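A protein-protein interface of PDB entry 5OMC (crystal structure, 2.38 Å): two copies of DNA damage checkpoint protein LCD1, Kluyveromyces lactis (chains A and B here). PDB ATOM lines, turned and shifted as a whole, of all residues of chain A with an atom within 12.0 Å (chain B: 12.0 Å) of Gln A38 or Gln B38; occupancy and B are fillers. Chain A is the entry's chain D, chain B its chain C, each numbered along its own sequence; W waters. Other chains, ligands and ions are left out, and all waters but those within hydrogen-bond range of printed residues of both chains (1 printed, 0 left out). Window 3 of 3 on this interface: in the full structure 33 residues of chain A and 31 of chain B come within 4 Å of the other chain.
O of Glu B36 lies within hydrogen-bond range of NE2 of Gln B41 (3.2 Å). The backbone carbonyl oxygen (O) of Glu A36 sits close to the side-chain amide oxygen (OE1) of Gln A41 (3.5 Å).
Among the printed residues, merely in contact across the chains: Gln A38 with Gln B38, Gln A38 with Ala B39, Ala A39 with Gln B38, Gln A41 with Leu B42, Leu A42 with Gln B41, Leu A42 with Leu B42, Ala A45 with Ala B45, Lys A46 with Gln B41, Val A49 with Ala B45 and Val A49 with Glu B48.
Ser A37 touches none of the printed residues of chain B. Of chain B, only Gln B38 comes within 4 Å of Ala A39. Gln A41 touches just one residue of chain B: Leu B42. Leu A42 touches just these residues of chain B: Gln B41 (3.6 Å) and Leu B42 (3.6 Å). Of the printed residues of chain B, Lys A46 touches Gln B41 (3.7 Å). Of the printed residues of chain B, Val A49 touches Ala B45 and Glu B48. Pro B34 touches none of the printed residues of chain A. No residue of chain A comes within 4 Å of Ser B37. Gln B38 touches two residues of chain A. Glu B40 touches none of the printed residues of chain A. Gln B41 touches just these residues of chain A: Leu A42 and Lys A46. Printed residues of chain A within 4 Å of Leu B42: Gln A41 (3.6 Å) and Leu A42 (3.6 Å). Printed residues of chain A within 4 Å of Ala B45: Ala A45 and Val A49.
Among the printed residues, no Asp or Glu carboxylate lies within 4 Å of a Lys or Arg side-chain nitrogen of the other chain.
Gln A38 touches its own counterpart, Gln B38. Gln A41 touches Leu B42, and with the chains exchanged Leu A42 touches Gln B41. Leu B42 touches its own counterpart, Leu A42. Ala A45 touches its own counterpart, Ala B45.
Water W1 lies within hydrogen-bond range of the backbone carbonyl oxygen of Gln B41 and the side-chain amino group of Lys A46.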
ATOM      1  N   LYS A  33      16.677  31.487  26.922  1.00  0.00           N
ATOM      2  CA  LYS A  33      16.225  30.150  26.531  1.00  0.00           C
ATOM      3  C   LYS A  33      17.416  29.145  26.564  1.00  0.00           C
ATOM      4  O   LYS A  33      18.533  29.501  26.158  1.00  0.00           O
ATOM      5  CB  LYS A  33      15.582  30.178  25.119  1.00  0.00           C
ATOM      6  CG  LYS A  33      14.141  30.700  25.090  1.00  0.00           C
ATOM      7  CD  LYS A  33      13.777  31.303  23.724  1.00  0.00           C
ATOM      8  CE  LYS A  33      12.463  32.062  23.743  1.00  0.00           C
ATOM      9  NZ  LYS A  33      12.117  32.631  22.406  1.00  0.00           N
ATOM     10  N   PRO A  34      17.195  27.919  27.121  1.00  0.00           N
ATOM     11  CA  PRO A  34      18.262  26.903  27.125  1.00  0.00           C
ATOM     12  C   PRO A  34      18.722  26.620  25.681  1.00  0.00           C
ATOM     13  O   PRO A  34      17.883  26.660  24.773  1.00  0.00           O
ATOM     14  CB  PRO A  34      17.590  25.682  27.771  1.00  0.00           C
ATOM     15  CG  PRO A  34      16.448  26.232  28.532  1.00  0.00           C
ATOM     16  CD  PRO A  34      15.947  27.363  27.680  1.00  0.00           C
ATOM     17  N   PRO A  35      20.052  26.435  25.446  1.00  0.00           N
ATOM     18  CA  PRO A  35      20.565  26.276  24.073  1.00  0.00           C
ATOM     19  C   PRO A  35      19.776  25.328  23.164  1.00  0.00           C
ATOM     20  O   PRO A  35      19.347  24.238  23.568  1.00  0.00           O
ATOM     21  CB  PRO A  35      21.999  25.808  24.283  1.00  0.00           C
ATOM     22  CG  PRO A  35      22.374  26.390  25.559  1.00  0.00           C
ATOM     23  CD  PRO A  35      21.152  26.390  26.421  1.00  0.00           C
ATOM     24  N   GLU A  36      19.554  25.801  21.943  1.00  0.00           N
ATOM     25  CA  GLU A  36      18.822  25.061  20.946  1.00  0.00           C
ATOM     26  C   GLU A  36      19.743  24.724  19.810  1.00  0.00           C
ATOM     27  O   GLU A  36      20.563  25.554  19.402  1.00  0.00           O
ATOM     28  CB  GLU A  36      17.643  25.880  20.434  1.00  0.00           C
ATOM     29  CG  GLU A  36      16.567  26.186  21.464  1.00  0.00           C
ATOM     30  CD  GLU A  36      15.238  26.486  20.815  1.00  0.00           C
ATOM     31  OE1 GLU A  36      15.229  27.112  19.731  1.00  0.00           O
ATOM     32  OE2 GLU A  36      14.204  26.046  21.364  1.00  0.00           O
ATOM     33  N   SER A  37      19.621  23.494  19.302  1.00  0.00           N
ATOM     34  CA  SER A  37      20.414  23.028  18.165  1.00  0.00           C
ATOM     35  C   SER A  37      19.954  23.752  16.930  1.00  0.00           C
ATOM     36  O   SER A  37      18.823  24.247  16.888  1.00  0.00           O
ATOM     37  CB  SER A  37      20.221  21.529  17.959  1.00  0.00           C
ATOM     38  OG  SER A  37      18.937  21.196  17.457  1.00  0.00           O
ATOM     39  N   GLN A  38      20.806  23.792  15.922  1.00  0.00           N
ATOM     40  CA  GLN A  38      20.493  24.378  14.615  1.00  0.00           C
ATOM     41  C   GLN A  38      19.188  23.769  14.040  1.00  0.00           C
ATOM     42  O   GLN A  38      18.355  24.517  13.552  1.00  0.00           O
ATOM     43  CB  GLN A  38      21.646  24.169  13.637  1.00  0.00           C
ATOM     44  CG  GLN A  38      22.872  24.997  13.945  1.00  0.00           C
ATOM     45  CD  GLN A  38      23.798  24.953  12.767  1.00  0.00           C
ATOM     46  OE1 GLN A  38      24.168  23.883  12.258  1.00  0.00           O
ATOM     47  NE2 GLN A  38      24.167  26.118  12.288  1.00  0.00           N
ATOM     48  N   ALA A  39      18.980  22.454  14.171  1.00  0.00           N
ATOM     49  CA  ALA A  39      17.756  21.784  13.707  1.00  0.00           C
ATOM     50  C   ALA A  39      16.469  22.295  14.388  1.00  0.00           C
ATOM     51  O   ALA A  39      15.440  22.452  13.707  1.00  0.00           O
ATOM     52  CB  ALA A  39      17.883  20.293  13.876  1.00  0.00           C
ATOM     53  N   GLU A  40      16.538  22.573  15.719  1.00  0.00           N
ATOM     54  CA  GLU A  40      15.424  23.111  16.525  1.00  0.00           C
ATOM     55  C   GLU A  40      15.157  24.546  16.123  1.00  0.00           C
ATOM     56  O   GLU A  40      14.020  24.980  15.974  1.00  0.00           O
ATOM     57  CB  GLU A  40      15.790  23.102  18.018  1.00  0.00           C
ATOM     58  CG  GLU A  40      15.897  21.738  18.650  1.00  0.00           C
ATOM     59  CD  GLU A  40      16.243  21.792  20.124  1.00  0.00           C
ATOM     60  OE1 GLU A  40      15.298  21.705  20.938  1.00  0.00           O
ATOM     61  OE2 GLU A  40      17.436  21.978  20.468  1.00  0.00           O
ATOM     62  N   GLN A  41      16.225  25.286  15.967  1.00  0.00           N
ATOM     63  CA  GLN A  41      16.163  26.666  15.564  1.00  0.00           C
ATOM     64  C   GLN A  41      15.661  26.842  14.149  1.00  0.00           C
ATOM     65  O   GLN A  41      14.911  27.769  13.912  1.00  0.00           O
ATOM     66  CB  GLN A  41      17.516  27.336  15.769  1.00  0.00           C
ATOM     67  CG  GLN A  41      17.681  27.789  17.205  1.00  0.00           C
ATOM     68  CD  GLN A  41      18.806  28.745  17.296  1.00  0.00           C
ATOM     69  OE1 GLN A  41      19.950  28.318  17.363  1.00  0.00           O
ATOM     70  NE2 GLN A  41      18.492  30.043  17.284  1.00  0.00           N
ATOM     71  N   LEU A  42      16.043  25.958  13.223  1.00  0.00           N
ATOM     72  CA  LEU A  42      15.608  26.023  11.821  1.00  0.00           C
ATOM     73  C   LEU A  42      14.094  25.779  11.716  1.00  0.00           C
ATOM     74  O   LEU A  42      13.421  26.490  10.982  1.00  0.00           O
ATOM     75  CB  LEU A  42      16.431  25.064  10.942  1.00  0.00           C
ATOM     76  CG  LEU A  42      16.209  25.072   9.436  1.00  0.00           C
ATOM     77  CD1 LEU A  42      16.384  26.480   8.839  1.00  0.00           C
ATOM     78  CD2 LEU A  42      17.081  24.048   8.768  1.00  0.00           C
ATOM     79  N   MET A  43      13.562  24.860  12.500  1.00  0.00           N
ATOM     80  CA  MET A  43      12.138  24.580  12.514  1.00  0.00           C
ATOM     81  C   MET A  43      11.330  25.780  12.994  1.00  0.00           C
ATOM     82  O   MET A  43      10.339  26.188  12.356  1.00  0.00           O
ATOM     83  CB  MET A  43      11.873  23.375  13.428  1.00  0.00           C
ATOM     84  CG  MET A  43      12.068  22.063  12.722  1.00  0.00           C
ATOM     85  SD  MET A  43      10.672  21.394  11.833  1.00  0.00           S
ATOM     86  CE  MET A  43       9.837  20.706  13.124  1.00  0.00           C
ATOM     87  N   LYS A  44      11.766  26.347  14.128  1.00  0.00           N
ATOM     88  CA  LYS A  44      11.157  27.532  14.699  1.00  0.00           C
ATOM     89  C   LYS A  44      11.229  28.707  13.739  1.00  0.00           C
ATOM     90  O   LYS A  44      10.200  29.342  13.456  1.00  0.00           O
ATOM     91  CB  LYS A  44      11.798  27.849  16.051  1.00  0.00           C
ATOM     92  CG  LYS A  44      11.219  26.994  17.191  1.00  0.00           C
ATOM     93  CD  LYS A  44      12.182  26.776  18.344  1.00  0.00           C
ATOM     94  CE  LYS A  44      11.517  26.101  19.517  1.00  0.00           C
ATOM     95  NZ  LYS A  44      11.624  26.923  20.764  1.00  0.00           N
ATOM     96  N   ALA A  45      12.415  28.947  13.160  1.00  0.00           N
ATOM     97  CA  ALA A  45      12.609  30.057  12.230  1.00  0.00           C
ATOM     98  C   ALA A  45      11.707  29.907  11.000  1.00  0.00           C
ATOM     99  O   ALA A  45      11.041  30.876  10.637  1.00  0.00           O
ATOM    100  CB  ALA A  45      14.075  30.186  11.839  1.00  0.00           C
ATOM    101  N   LYS A  46      11.610  28.684  10.422  1.00  0.00           N
ATOM    102  CA  LYS A  46      10.772  28.400   9.249  1.00  0.00           C
ATOM    103  C   LYS A  46       9.320  28.650   9.577  1.00  0.00           C
ATOM    104  O   LYS A  46       8.618  29.232   8.754  1.00  0.00           O
ATOM    105  CB  LYS A  46      10.978  26.983   8.718  1.00  0.00           C
ATOM    106  CG  LYS A  46      12.284  26.776   7.972  1.00  0.00           C
ATOM    107  CD  LYS A  46      12.060  26.747   6.489  1.00  0.00           C
ATOM    108  CE  LYS A  46      13.358  26.539   5.768  1.00  0.00           C
ATOM    109  NZ  LYS A  46      13.263  26.898   4.327  1.00  0.00           N
ATOM    110  N   GLY A  47       8.898  28.246  10.783  1.00  0.00           N
ATOM    111  CA  GLY A  47       7.557  28.492  11.279  1.00  0.00           C
ATOM    112  C   GLY A  47       7.287  29.985  11.389  1.00  0.00           C
ATOM    113  O   GLY A  47       6.242  30.450  10.941  1.00  0.00           O
ATOM    114  N   GLU A  48       8.231  30.750  11.966  1.00  0.00           N
ATOM    115  CA  GLU A  48       8.101  32.223  12.078  1.00  0.00           C
ATOM    116  C   GLU A  48       7.978  32.884  10.702  1.00  0.00           C
ATOM    117  O   GLU A  48       7.199  33.816  10.540  1.00  0.00           O
ATOM    118  CB  GLU A  48       9.300  32.849  12.808  1.00  0.00           C
ATOM    119  CG  GLU A  48       9.376  32.608  14.296  1.00  0.00           C
ATOM    120  CD  GLU A  48      10.566  33.309  14.926  1.00  0.00           C
ATOM    121  OE1 GLU A  48      10.599  34.562  14.902  1.00  0.00           O
ATOM    122  OE2 GLU A  48      11.493  32.604  15.390  1.00  0.00           O
ATOM    123  N   VAL A  49       8.762  32.412   9.730  1.00  0.00           N
ATOM    124  CA  VAL A  49       8.759  32.946   8.357  1.00  0.00           C
ATOM    125  C   VAL A  49       7.343  32.825   7.759  1.00  0.00           C
ATOM    126  O   VAL A  49       6.819  33.801   7.218  1.00  0.00           O
ATOM    127  CB  VAL A  49       9.874  32.309   7.448  1.00  0.00           C
ATOM    128  CG1 VAL A  49       9.659  32.597   5.953  1.00  0.00           C
ATOM    129  CG2 VAL A  49      11.260  32.770   7.882  1.00  0.00           C
ATOM    130  N   PRO B  34      20.213  23.939  -5.178  1.00  0.00           N
ATOM    131  CA  PRO B  34      21.457  23.335  -4.647  1.00  0.00           C
ATOM    132  C   PRO B  34      21.400  23.181  -3.138  1.00  0.00           C
ATOM    133  O   PRO B  34      20.902  24.104  -2.482  1.00  0.00           O
ATOM    134  CB  PRO B  34      22.571  24.277  -5.120  1.00  0.00           C
ATOM    135  CG  PRO B  34      21.954  25.091  -6.216  1.00  0.00           C
ATOM    136  CD  PRO B  34      20.495  25.210  -5.874  1.00  0.00           C
ATOM    137  N   PRO B  35      21.798  21.991  -2.591  1.00  0.00           N
ATOM    138  CA  PRO B  35      21.659  21.769  -1.131  1.00  0.00           C
ATOM    139  C   PRO B  35      22.280  22.855  -0.263  1.00  0.00           C
ATOM    140  O   PRO B  35      23.391  23.348  -0.541  1.00  0.00           O
ATOM    141  CB  PRO B  35      22.308  20.396  -0.890  1.00  0.00           C
ATOM    142  CG  PRO B  35      22.296  19.714  -2.211  1.00  0.00           C
ATOM    143  CD  PRO B  35      22.354  20.793  -3.273  1.00  0.00           C
ATOM    144  N   GLU B  36      21.531  23.253   0.769  1.00  0.00           N
ATOM    145  CA  GLU B  36      22.018  24.257   1.698  1.00  0.00           C
ATOM    146  C   GLU B  36      22.146  23.620   3.054  1.00  0.00           C
ATOM    147  O   GLU B  36      21.268  22.848   3.468  1.00  0.00           O
ATOM    148  CB  GLU B  36      21.079  25.447   1.776  1.00  0.00           C
ATOM    149  CG  GLU B  36      20.958  26.242   0.501  1.00  0.00           C
ATOM    150  CD  GLU B  36      20.497  27.660   0.773  1.00  0.00           C
ATOM    151  OE1 GLU B  36      19.645  27.858   1.674  1.00  0.00           O
ATOM    152  OE2 GLU B  36      21.029  28.578   0.108  1.00  0.00           O
ATOM    153  N   SER B  37      23.247  23.940   3.750  1.00  0.00           N
ATOM    154  CA  SER B  37      23.494  23.440   5.096  1.00  0.00           C
ATOM    155  C   SER B  37      22.494  24.074   6.043  1.00  0.00           C
ATOM    156  O   SER B  37      21.954  25.139   5.744  1.00  0.00           O
ATOM    157  CB  SER B  37      24.911  23.785   5.542  1.00  0.00           C
ATOM    158  OG  SER B  37      25.073  25.168   5.800  1.00  0.00           O
ATOM    159  N   GLN B  38      22.277  23.437   7.197  1.00  0.00           N
ATOM    160  CA  GLN B  38      21.407  23.945   8.253  1.00  0.00           C
ATOM    161  C   GLN B  38      21.806  25.380   8.643  1.00  0.00           C
ATOM    162  O   GLN B  38      20.937  26.233   8.772  1.00  0.00           O
ATOM    163  CB  GLN B  38      21.469  23.007   9.456  1.00  0.00           C
ATOM    164  CG  GLN B  38      20.765  21.673   9.223  1.00  0.00           C
ATOM    165  CD  GLN B  38      20.280  21.097  10.514  1.00  0.00           C
ATOM    166  OE1 GLN B  38      21.025  21.014  11.488  1.00  0.00           O
ATOM    167  NE2 GLN B  38      19.006  20.723  10.561  1.00  0.00           N
ATOM    168  N   ALA B  39      23.114  25.660   8.735  1.00  0.00           N
ATOM    169  CA  ALA B  39      23.650  26.990   9.051  1.00  0.00           C
ATOM    170  C   ALA B  39      23.248  28.054   8.031  1.00  0.00           C
ATOM    171  O   ALA B  39      22.920  29.158   8.434  1.00  0.00           O
ATOM    172  CB  ALA B  39      25.168  26.931   9.170  1.00  0.00           C
ATOM    173  N   GLU B  40      23.266  27.715   6.721  1.00  0.00           N
ATOM    174  CA  GLU B  40      22.893  28.602   5.606  1.00  0.00           C
ATOM    175  C   GLU B  40      21.395  28.828   5.646  1.00  0.00           C
ATOM    176  O   GLU B  40      20.927  29.939   5.440  1.00  0.00           O
ATOM    177  CB  GLU B  40      23.225  27.967   4.253  1.00  0.00           C
ATOM    178  CG  GLU B  40      24.700  27.868   3.946  1.00  0.00           C
ATOM    179  CD  GLU B  40      24.968  27.216   2.608  1.00  0.00           C
ATOM    180  OE1 GLU B  40      25.180  25.980   2.577  1.00  0.00           O
ATOM    181  OE2 GLU B  40      24.918  27.934   1.586  1.00  0.00           O
ATOM    182  N   GLN B  41      20.650  27.775   5.874  1.00  0.00           N
ATOM    183  CA  GLN B  41      19.214  27.849   5.942  1.00  0.00           C
ATOM    184  C   GLN B  41      18.707  28.646   7.156  1.00  0.00           C
ATOM    185  O   GLN B  41      17.751  29.426   7.035  1.00  0.00           O
ATOM    186  CB  GLN B  41      18.643  26.438   5.910  1.00  0.00           C
ATOM    187  CG  GLN B  41      18.536  25.913   4.496  1.00  0.00           C
ATOM    188  CD  GLN B  41      17.633  24.721   4.492  1.00  0.00           C
ATOM    189  OE1 GLN B  41      16.391  24.826   4.641  1.00  0.00           O
ATOM    190  NE2 GLN B  41      18.247  23.555   4.410  1.00  0.00           N
ATOM    191  N   LEU B  42      19.360  28.491   8.303  1.00  0.00           N
ATOM    192  CA  LEU B  42      18.998  29.209   9.520  1.00  0.00           C
ATOM    193  C   LEU B  42      19.260  30.717   9.374  1.00  0.00           C
ATOM    194  O   LEU B  42      18.436  31.529   9.796  1.00  0.00           O
ATOM    195  CB  LEU B  42      19.721  28.580  10.737  1.00  0.00           C
ATOM    196  CG  LEU B  42      19.357  29.060  12.147  1.00  0.00           C
ATOM    197  CD1 LEU B  42      17.884  29.025  12.415  1.00  0.00           C
ATOM    198  CD2 LEU B  42      20.008  28.203  13.145  1.00  0.00           C
ATOM    199  N   MET B  43      20.367  31.083   8.720  1.00  0.00           N
ATOM    200  CA  MET B  43      20.722  32.476   8.458  1.00  0.00           C
ATOM    201  C   MET B  43      19.719  33.122   7.558  1.00  0.00           C
ATOM    202  O   MET B  43      19.294  34.240   7.862  1.00  0.00           O
ATOM    203  CB  MET B  43      22.054  32.564   7.789  1.00  0.00           C
ATOM    204  CG  MET B  43      23.110  32.788   8.727  1.00  0.00           C
ATOM    205  SD  MET B  43      24.189  33.971   7.913  1.00  0.00           S
ATOM    206  CE  MET B  43      25.114  32.819   6.946  1.00  0.00           C
ATOM    207  N   LYS B  44      19.345  32.446   6.451  1.00  0.00           N
ATOM    208  CA  LYS B  44      18.342  32.918   5.509  1.00  0.00           C
ATOM    209  C   LYS B  44      17.019  33.089   6.199  1.00  0.00           C
ATOM    210  O   LYS B  44      16.434  34.161   6.101  1.00  0.00           O
ATOM    211  CB  LYS B  44      18.232  31.989   4.298  1.00  0.00           C
ATOM    212  CG  LYS B  44      19.303  32.331   3.257  1.00  0.00           C
ATOM    213  CD  LYS B  44      19.713  31.154   2.384  1.00  0.00           C
ATOM    214  CE  LYS B  44      20.700  31.569   1.305  1.00  0.00           C
ATOM    215  NZ  LYS B  44      22.014  30.874   1.470  1.00  0.00           N
ATOM    216  N   ALA B  45      16.584  32.099   6.986  1.00  0.00           N
ATOM    217  CA  ALA B  45      15.309  32.201   7.688  1.00  0.00           C
ATOM    218  C   ALA B  45      15.294  33.417   8.644  1.00  0.00           C
ATOM    219  O   ALA B  45      14.363  34.233   8.598  1.00  0.00           O
ATOM    220  CB  ALA B  45      15.007  30.899   8.422  1.00  0.00           C
ATOM    221  N   LYS B  46      16.373  33.591   9.430  1.00  0.00           N
ATOM    222  CA  LYS B  46      16.525  34.715  10.383  1.00  0.00           C
ATOM    223  C   LYS B  46      16.518  36.058   9.661  1.00  0.00           C
ATOM    224  O   LYS B  46      15.863  37.001  10.106  1.00  0.00           O
ATOM    225  CB  LYS B  46      17.784  34.536  11.278  1.00  0.00           C
ATOM    226  CG  LYS B  46      17.706  33.380  12.311  1.00  0.00           C
ATOM    227  CD  LYS B  46      16.847  33.698  13.579  1.00  0.00           C
ATOM    228  CE  LYS B  46      16.792  32.523  14.517  1.00  0.00           C
ATOM    229  NZ  LYS B  46      16.068  32.871  15.756  1.00  0.00           N
ATOM    230  N   GLY B  47      17.192  36.108   8.516  1.00  0.00           N
ATOM    231  CA  GLY B  47      17.209  37.284   7.659  1.00  0.00           C
ATOM    232  C   GLY B  47      15.836  37.598   7.112  1.00  0.00           C
ATOM    233  O   GLY B  47      15.434  38.762   7.148  1.00  0.00           O
ATOM    234  N   GLU B  48      15.081  36.559   6.634  1.00  0.00           N
ATOM    235  CA  GLU B  48      13.694  36.713   6.157  1.00  0.00           C
ATOM    236  C   GLU B  48      12.793  37.236   7.271  1.00  0.00           C
ATOM    237  O   GLU B  48      11.922  38.059   6.998  1.00  0.00           O
ATOM    238  CB  GLU B  48      13.103  35.409   5.652  1.00  0.00           C
ATOM    239  CG  GLU B  48      13.610  34.926   4.313  1.00  0.00           C
ATOM    240  CD  GLU B  48      12.886  33.668   3.863  1.00  0.00           C
ATOM    241  OE1 GLU B  48      11.707  33.808   3.464  1.00  0.00           O
ATOM    242  OE2 GLU B  48      13.471  32.556   3.925  1.00  0.00           O
HETATM  243  O   HOH W   1      15.469  29.156   5.337  1.00  0.00           O
